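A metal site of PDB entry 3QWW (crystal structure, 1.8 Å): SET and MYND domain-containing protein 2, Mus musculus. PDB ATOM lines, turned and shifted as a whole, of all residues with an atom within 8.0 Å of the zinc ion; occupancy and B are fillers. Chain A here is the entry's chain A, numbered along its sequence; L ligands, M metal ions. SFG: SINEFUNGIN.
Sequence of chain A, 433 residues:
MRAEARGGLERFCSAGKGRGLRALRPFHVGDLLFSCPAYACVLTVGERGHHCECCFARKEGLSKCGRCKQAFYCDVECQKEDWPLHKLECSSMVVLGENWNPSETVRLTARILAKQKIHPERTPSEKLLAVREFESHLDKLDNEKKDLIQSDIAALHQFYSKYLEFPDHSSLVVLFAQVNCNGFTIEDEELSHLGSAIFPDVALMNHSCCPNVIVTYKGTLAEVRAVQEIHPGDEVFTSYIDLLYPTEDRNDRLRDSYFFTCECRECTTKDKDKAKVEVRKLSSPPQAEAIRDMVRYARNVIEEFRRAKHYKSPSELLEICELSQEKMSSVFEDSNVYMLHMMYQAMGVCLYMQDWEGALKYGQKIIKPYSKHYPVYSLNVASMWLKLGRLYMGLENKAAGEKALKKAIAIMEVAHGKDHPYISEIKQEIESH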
ATOM      1  N   HIS A 207       1.953  30.887  13.311  1.00  0.00           N
ATOM      2  CA  HIS A 207       3.200  30.133  13.135  1.00  0.00           C
ATOM      3  C   HIS A 207       3.166  28.772  13.765  1.00  0.00           C
ATOM      4  O   HIS A 207       2.641  28.587  14.871  1.00  0.00           O
ATOM      5  CB  HIS A 207       4.373  30.920  13.747  1.00  0.00           C
ATOM      6  CG  HIS A 207       5.637  30.105  13.872  1.00  0.00           C
ATOM      7  ND1 HIS A 207       6.488  29.953  12.797  1.00  0.00           N
ATOM      8  CD2 HIS A 207       6.076  29.305  14.888  1.00  0.00           C
ATOM      9  CE1 HIS A 207       7.458  29.147  13.199  1.00  0.00           C
ATOM     10  NE2 HIS A 207       7.224  28.681  14.435  1.00  0.00           N
ATOM     11  N   SER A 208       3.858  27.827  13.117  1.00  0.00           N
ATOM     12  CA  SER A 208       4.180  26.541  13.682  1.00  0.00           C
ATOM     13  C   SER A 208       5.557  26.132  13.134  1.00  0.00           C
ATOM     14  O   SER A 208       5.875  26.415  11.976  1.00  0.00           O
ATOM     15  CB  SER A 208       3.157  25.475  13.335  1.00  0.00           C
ATOM     16  OG  SER A 208       3.558  24.266  13.963  1.00  0.00           O
ATOM     17  N   CYS A 209       6.339  25.393  13.941  1.00  0.00           N
ATOM     18  CA  CYS A 209       7.627  24.843  13.486  1.00  0.00           C
ATOM     19  C   CYS A 209       7.368  23.545  12.690  1.00  0.00           C
ATOM     20  O   CYS A 209       8.313  22.971  12.148  1.00  0.00           O
ATOM     21  CB  CYS A 209       8.582  24.642  14.662  1.00  0.00           C
ATOM     22  SG  CYS A 209       8.878  26.159  15.631  1.00  0.00           S
ATOM     23  N   CYS A 210       6.101  23.105  12.635  1.00  0.00           N
ATOM     24  CA  CYS A 210       5.611  21.955  11.879  1.00  0.00           C
ATOM     25  C   CYS A 210       4.509  22.552  10.975  1.00  0.00           C
ATOM     26  O   CYS A 210       3.333  22.281  11.215  1.00  0.00           O
ATOM     27  CB  CYS A 210       5.056  20.881  12.823  1.00  0.00           C
ATOM     28  SG  CYS A 210       6.202  20.370  14.119  1.00  0.00           S
ATOM     29  N   SER A 239       5.488  28.733   8.636  1.00  0.00           N
ATOM     30  CA  SER A 239       6.613  28.938   9.565  1.00  0.00           C
ATOM     31  C   SER A 239       7.123  30.365   9.284  1.00  0.00           C
ATOM     32  O   SER A 239       7.363  30.715   8.114  1.00  0.00           O
ATOM     33  CB  SER A 239       7.745  27.949   9.336  1.00  0.00           C
ATOM     34  OG  SER A 239       8.835  28.372  10.155  1.00  0.00           O
ATOM     35  N   ILE A 241       9.964  31.474  10.411  1.00  0.00           N
ATOM     36  CA  ILE A 241      11.405  31.460  10.551  1.00  0.00           C
ATOM     37  C   ILE A 241      12.068  30.259   9.906  1.00  0.00           C
ATOM     38  O   ILE A 241      11.400  29.309   9.481  1.00  0.00           O
ATOM     39  CB  ILE A 241      11.732  31.500  12.083  1.00  0.00           C
ATOM     40  CG1 ILE A 241      10.965  30.387  12.848  1.00  0.00           C
ATOM     41  CG2 ILE A 241      11.495  32.897  12.727  1.00  0.00           C
ATOM     42  CD1 ILE A 241      11.728  29.869  13.915  1.00  0.00           C
ATOM     43  N   LEU A 243      13.662  26.942   9.869  1.00  0.00           N
ATOM     44  CA  LEU A 243      13.461  25.762  10.700  1.00  0.00           C
ATOM     45  C   LEU A 243      14.725  24.959  10.948  1.00  0.00           C
ATOM     46  O   LEU A 243      14.685  23.992  11.715  1.00  0.00           O
ATOM     47  CB  LEU A 243      12.352  24.881  10.102  1.00  0.00           C
ATOM     48  CG  LEU A 243      10.959  25.498  10.064  1.00  0.00           C
ATOM     49  CD1 LEU A 243       9.996  24.592   9.270  1.00  0.00           C
ATOM     50  CD2 LEU A 243      10.436  25.819  11.479  1.00  0.00           C
ATOM     51  N   THR A 247      15.546  24.348  18.974  1.00  0.00           N
ATOM     52  CA  THR A 247      14.383  24.974  19.629  1.00  0.00           C
ATOM     53  C   THR A 247      14.649  26.320  20.297  1.00  0.00           C
ATOM     54  O   THR A 247      13.885  27.262  20.103  1.00  0.00           O
ATOM     55  CB  THR A 247      13.755  23.962  20.591  1.00  0.00           C
ATOM     56  OG1 THR A 247      13.469  22.760  19.865  1.00  0.00           O
ATOM     57  CG2 THR A 247      12.471  24.493  21.269  1.00  0.00           C
ATOM     58  N   ARG A 250      15.181  29.115  17.645  1.00  0.00           N
ATOM     59  CA  ARG A 250      13.906  29.451  16.972  1.00  0.00           C
ATOM     60  C   ARG A 250      13.053  30.318  17.894  1.00  0.00           C
ATOM     61  O   ARG A 250      12.528  31.334  17.447  1.00  0.00           O
ATOM     62  CB  ARG A 250      13.126  28.201  16.609  1.00  0.00           C
ATOM     63  CG  ARG A 250      13.814  27.336  15.526  1.00  0.00           C
ATOM     64  CD  ARG A 250      12.835  26.331  14.931  1.00  0.00           C
ATOM     65  NE  ARG A 250      12.064  25.586  15.923  1.00  0.00           N
ATOM     66  CZ  ARG A 250      12.483  24.485  16.544  1.00  0.00           C
ATOM     67  NH1 ARG A 250      13.703  24.003  16.307  1.00  0.00           N
ATOM     68  NH2 ARG A 250      11.693  23.865  17.409  1.00  0.00           N
ATOM     69  N   ASN A 251      12.927  29.926  19.183  1.00  0.00           N
ATOM     70  CA  ASN A 251      12.110  30.685  20.121  1.00  0.00           C
ATOM     71  C   ASN A 251      12.653  32.046  20.506  1.00  0.00           C
ATOM     72  O   ASN A 251      11.874  32.971  20.715  1.00  0.00           O
ATOM     73  CB  ASN A 251      11.659  29.854  21.289  1.00  0.00           C
ATOM     74  CG  ASN A 251      10.489  28.982  20.935  1.00  0.00           C
ATOM     75  OD1 ASN A 251       9.402  29.477  20.615  1.00  0.00           O
ATOM     76  ND2 ASN A 251      10.716  27.673  20.898  1.00  0.00           N
ATOM     77  N   LEU A 254      11.469  34.043  17.548  1.00  0.00           N
ATOM     78  CA  LEU A 254      10.029  34.284  17.618  1.00  0.00           C
ATOM     79  C   LEU A 254       9.688  35.312  18.684  1.00  0.00           C
ATOM     80  O   LEU A 254       8.910  36.204  18.410  1.00  0.00           O
ATOM     81  CB  LEU A 254       9.256  32.967  17.837  1.00  0.00           C
ATOM     82  CG  LEU A 254       9.314  32.009  16.611  1.00  0.00           C
ATOM     83  CD1 LEU A 254       8.803  30.615  16.980  1.00  0.00           C
ATOM     84  CD2 LEU A 254       8.539  32.591  15.383  1.00  0.00           C
ATOM     85  N   PHE A 260       6.107  36.157  21.003  1.00  0.00           N
ATOM     86  CA  PHE A 260       5.446  34.962  21.519  1.00  0.00           C
ATOM     87  C   PHE A 260       6.465  33.831  21.587  1.00  0.00           C
ATOM     88  O   PHE A 260       7.447  33.849  20.853  1.00  0.00           O
ATOM     89  CB  PHE A 260       4.223  34.505  20.674  1.00  0.00           C
ATOM     90  CG  PHE A 260       4.560  33.822  19.358  1.00  0.00           C
ATOM     91  CD1 PHE A 260       4.751  34.563  18.197  1.00  0.00           C
ATOM     92  CD2 PHE A 260       4.693  32.432  19.284  1.00  0.00           C
ATOM     93  CE1 PHE A 260       5.043  33.926  16.976  1.00  0.00           C
ATOM     94  CE2 PHE A 260       5.016  31.805  18.071  1.00  0.00           C
ATOM     95  CZ  PHE A 260       5.188  32.556  16.931  1.00  0.00           C
ATOM     96  N   THR A 261       6.170  32.842  22.406  1.00  0.00           N
ATOM     97  CA  THR A 261       6.937  31.612  22.519  1.00  0.00           C
ATOM     98  C   THR A 261       6.119  30.492  21.874  1.00  0.00           C
ATOM     99  O   THR A 261       4.942  30.307  22.206  1.00  0.00           O
ATOM    100  CB  THR A 261       7.216  31.280  23.988  1.00  0.00           C
ATOM    101  OG1 THR A 261       8.085  32.294  24.505  1.00  0.00           O
ATOM    102  CG2 THR A 261       7.863  29.881  24.155  1.00  0.00           C
ATOM    103  N   CYS A 262       6.731  29.769  20.934  1.00  0.00           N
ATOM    104  CA  CYS A 262       6.032  28.692  20.254  1.00  0.00           C
ATOM    105  C   CYS A 262       5.819  27.483  21.155  1.00  0.00           C
ATOM    106  O   CYS A 262       6.730  27.094  21.874  1.00  0.00           O
ATOM    107  CB  CYS A 262       6.774  28.285  18.974  1.00  0.00           C
ATOM    108  SG  CYS A 262       5.868  27.109  17.954  1.00  0.00           S
ATOM    109  N   GLU A 263       4.648  26.854  21.068  1.00  0.00           N
ATOM    110  CA  GLU A 263       4.318  25.645  21.841  1.00  0.00           C
ATOM    111  C   GLU A 263       3.963  24.466  20.936  1.00  0.00           C
ATOM    112  O   GLU A 263       3.231  23.564  21.346  1.00  0.00           O
ATOM    113  CB  GLU A 263       3.159  25.950  22.829  1.00  0.00           C
ATOM    114  CG  GLU A 263       3.567  26.850  23.981  1.00  0.00           C
ATOM    115  CD  GLU A 263       2.452  27.058  24.987  1.00  0.00           C
ATOM    116  OE1 GLU A 263       2.227  26.155  25.831  1.00  0.00           O
ATOM    117  OE2 GLU A 263       1.762  28.096  24.903  1.00  0.00           O
ATOM    118  N   CYS A 264       4.481  24.456  19.684  1.00  0.00           N
ATOM    119  CA  CYS A 264       4.194  23.369  18.749  1.00  0.00           C
ATOM    120  C   CYS A 264       4.846  22.047  19.256  1.00  0.00           C
ATOM    121  O   CYS A 264       5.638  22.071  20.200  1.00  0.00           O
ATOM    122  CB  CYS A 264       4.629  23.715  17.334  1.00  0.00           C
ATOM    123  SG  CYS A 264       6.411  23.622  17.041  1.00  0.00           S
ATOM    124  N   ARG A 265       4.516  20.937  18.625  1.00  0.00           N
ATOM    125  CA  ARG A 265       5.042  19.603  18.941  1.00  0.00           C
ATOM    126  C   ARG A 265       6.572  19.578  18.933  1.00  0.00           C
ATOM    127  O   ARG A 265       7.159  19.036  19.865  1.00  0.00           O
ATOM    128  CB  ARG A 265       4.454  18.543  17.981  1.00  0.00           C
ATOM    129  CG  ARG A 265       4.971  17.129  18.212  1.00  0.00           C
ATOM    130  CD  ARG A 265       4.112  16.331  19.179  1.00  0.00           C
ATOM    131  NE  ARG A 265       4.663  15.002  19.410  1.00  0.00           N
ATOM    132  CZ  ARG A 265       4.628  14.364  20.579  1.00  0.00           C
ATOM    133  NH1 ARG A 265       4.097  14.960  21.639  1.00  0.00           N
ATOM    134  NH2 ARG A 265       5.155  13.158  20.706  1.00  0.00           N
ATOM    135  N   GLU A 266       7.211  20.180  17.905  1.00  0.00           N
ATOM    136  CA  GLU A 266       8.666  20.227  17.793  1.00  0.00           C
ATOM    137  C   GLU A 266       9.276  21.041  18.934  1.00  0.00           C
ATOM    138  O   GLU A 266      10.346  20.681  19.422  1.00  0.00           O
ATOM    139  CB  GLU A 266       9.099  20.759  16.416  1.00  0.00           C
ATOM    140  CG  GLU A 266      10.610  20.701  16.152  1.00  0.00           C
ATOM    141  CD  GLU A 266      11.330  19.392  16.483  1.00  0.00           C
ATOM    142  OE1 GLU A 266      10.864  18.329  16.009  1.00  0.00           O
ATOM    143  OE2 GLU A 266      12.348  19.435  17.208  1.00  0.00           O
ATOM    144  N   CYS A 267       8.597  22.131  19.362  1.00  0.00           N
ATOM    145  CA  CYS A 267       9.091  22.960  20.452  1.00  0.00           C
ATOM    146  C   CYS A 267       8.882  22.320  21.799  1.00  0.00           C
ATOM    147  O   CYS A 267       9.663  22.567  22.711  1.00  0.00           O
ATOM    148  CB  CYS A 267       8.473  24.355  20.380  1.00  0.00           C
ATOM    149  SG  CYS A 267       9.167  25.362  19.045  1.00  0.00           S
ATOM    150  N   THR A 268       7.854  21.460  21.887  1.00  0.00           N
ATOM    151  CA  THR A 268       7.505  20.764  23.142  1.00  0.00           C
ATOM    152  C   THR A 268       8.422  19.547  23.346  1.00  0.00           C
ATOM    153  O   THR A 268       8.941  19.376  24.444  1.00  0.00           O
ATOM    154  CB  THR A 268       5.984  20.461  23.164  1.00  0.00           C
ATOM    155  OG1 THR A 268       5.305  21.717  23.166  1.00  0.00           O
ATOM    156  CG2 THR A 268       5.565  19.688  24.400  1.00  0.00           C
HETATM  157  N   SFG L   1      -2.679  35.965  15.320  1.00  0.00           N
HETATM  158  CA  SFG L   1      -2.340  37.230  14.550  1.00  0.00           C
HETATM  159  C   SFG L   1      -3.429  38.286  14.522  1.00  0.00           C
HETATM  160  O   SFG L   1      -4.460  38.103  15.255  1.00  0.00           O
HETATM  161  OXT SFG L   1      -3.350  39.295  13.790  1.00  0.00           O
HETATM  162  CB  SFG L   1      -2.075  36.778  13.050  1.00  0.00           C
HETATM  163  CG  SFG L   1      -0.522  36.446  12.875  1.00  0.00           C
HETATM  164  CD  SFG L   1       0.389  37.750  12.936  1.00  0.00           C
HETATM  165  NE  SFG L   1       1.067  37.972  11.629  1.00  0.00           N
HETATM  166  C5' SFG L   1       1.592  37.573  13.911  1.00  0.00           C
HETATM  167  C4' SFG L   1       1.245  37.379  15.461  1.00  0.00           C
HETATM  168  O4' SFG L   1       0.343  36.304  15.820  1.00  0.00           O
HETATM  169  C3' SFG L   1       2.407  37.229  16.358  1.00  0.00           C
HETATM  170  O3' SFG L   1       3.076  38.494  16.586  1.00  0.00           O
HETATM  171  C2' SFG L   1       1.767  36.673  17.655  1.00  0.00           C
HETATM  172  O2' SFG L   1       1.025  37.756  18.354  1.00  0.00           O
HETATM  173  C1' SFG L   1       0.701  35.759  17.085  1.00  0.00           C
HETATM  174  N9  SFG L   1       1.134  34.356  16.823  1.00  0.00           N
HETATM  175  C8  SFG L   1       1.541  33.794  15.572  1.00  0.00           C
HETATM  176  N7  SFG L   1       1.785  32.521  15.724  1.00  0.00           N
HETATM  177  C5  SFG L   1       1.621  32.277  17.090  1.00  0.00           C
HETATM  178  C6  SFG L   1       1.777  31.097  17.886  1.00  0.00           C
HETATM  179  N6  SFG L   1       2.172  29.919  17.333  1.00  0.00           N
HETATM  180  N1  SFG L   1       1.568  31.138  19.331  1.00  0.00           N
HETATM  181  C2  SFG L   1       1.163  32.375  19.837  1.00  0.00           C
HETATM  182  N3  SFG L   1       0.928  33.558  19.124  1.00  0.00           N
HETATM  183  C4  SFG L   1       1.204  33.413  17.756  1.00  0.00           C
HETATM  184 ZN    ZN M   1       7.487  25.567  17.491  1.00  0.00          ZN
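The backbone carbonyl oxygen (O) of His 207 lies within hydrogen-bond range of a nitrogen (N6) of the ligand, at 2.8 Å.
A nitrogen (N7) of the ligand is in hydrogen-bond range of the backbone NH (N) of His 207 (2.9 Å).
The side-chain hydroxyl (OG1) of Thr 268 is in hydrogen-bond range of the backbone carbonyl oxygen (O) of Cys 264 (3.0 Å).
NH2 of Arg 250 lies close to SG of Cys 267 (3.4 Å).
N of Glu 266 lies close to SG of Cys 264 (3.6 Å).
SG of Cys 209 lies close to NE of Arg 250 (3.3 Å).
OD1 of Asn 251 lies within hydrogen-bond range of N of Cys 262, 2.7 Å away.
SG of Cys 267 sits close to ND2 of Asn 251 (3.3 Å).
The backbone NH (N) of Cys 209 sits at hydrogen-bond distance from a ring nitrogen (NE2) of His 207 (3.4 Å).
Of the 20 residues printed, 4 come within 4 Å of the zinc ion.
The zinc ion is bound by SG of Cys 264, at 2.3 Å.
The zinc ion is bound by the side-chain sulfur (SG) of Cys 262 (2.3 Å).
SG of Cys 267 binds the zinc ion, at 2.3 Å.
The side-chain sulfur (SG) of Cys 209 binds the zinc ion.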
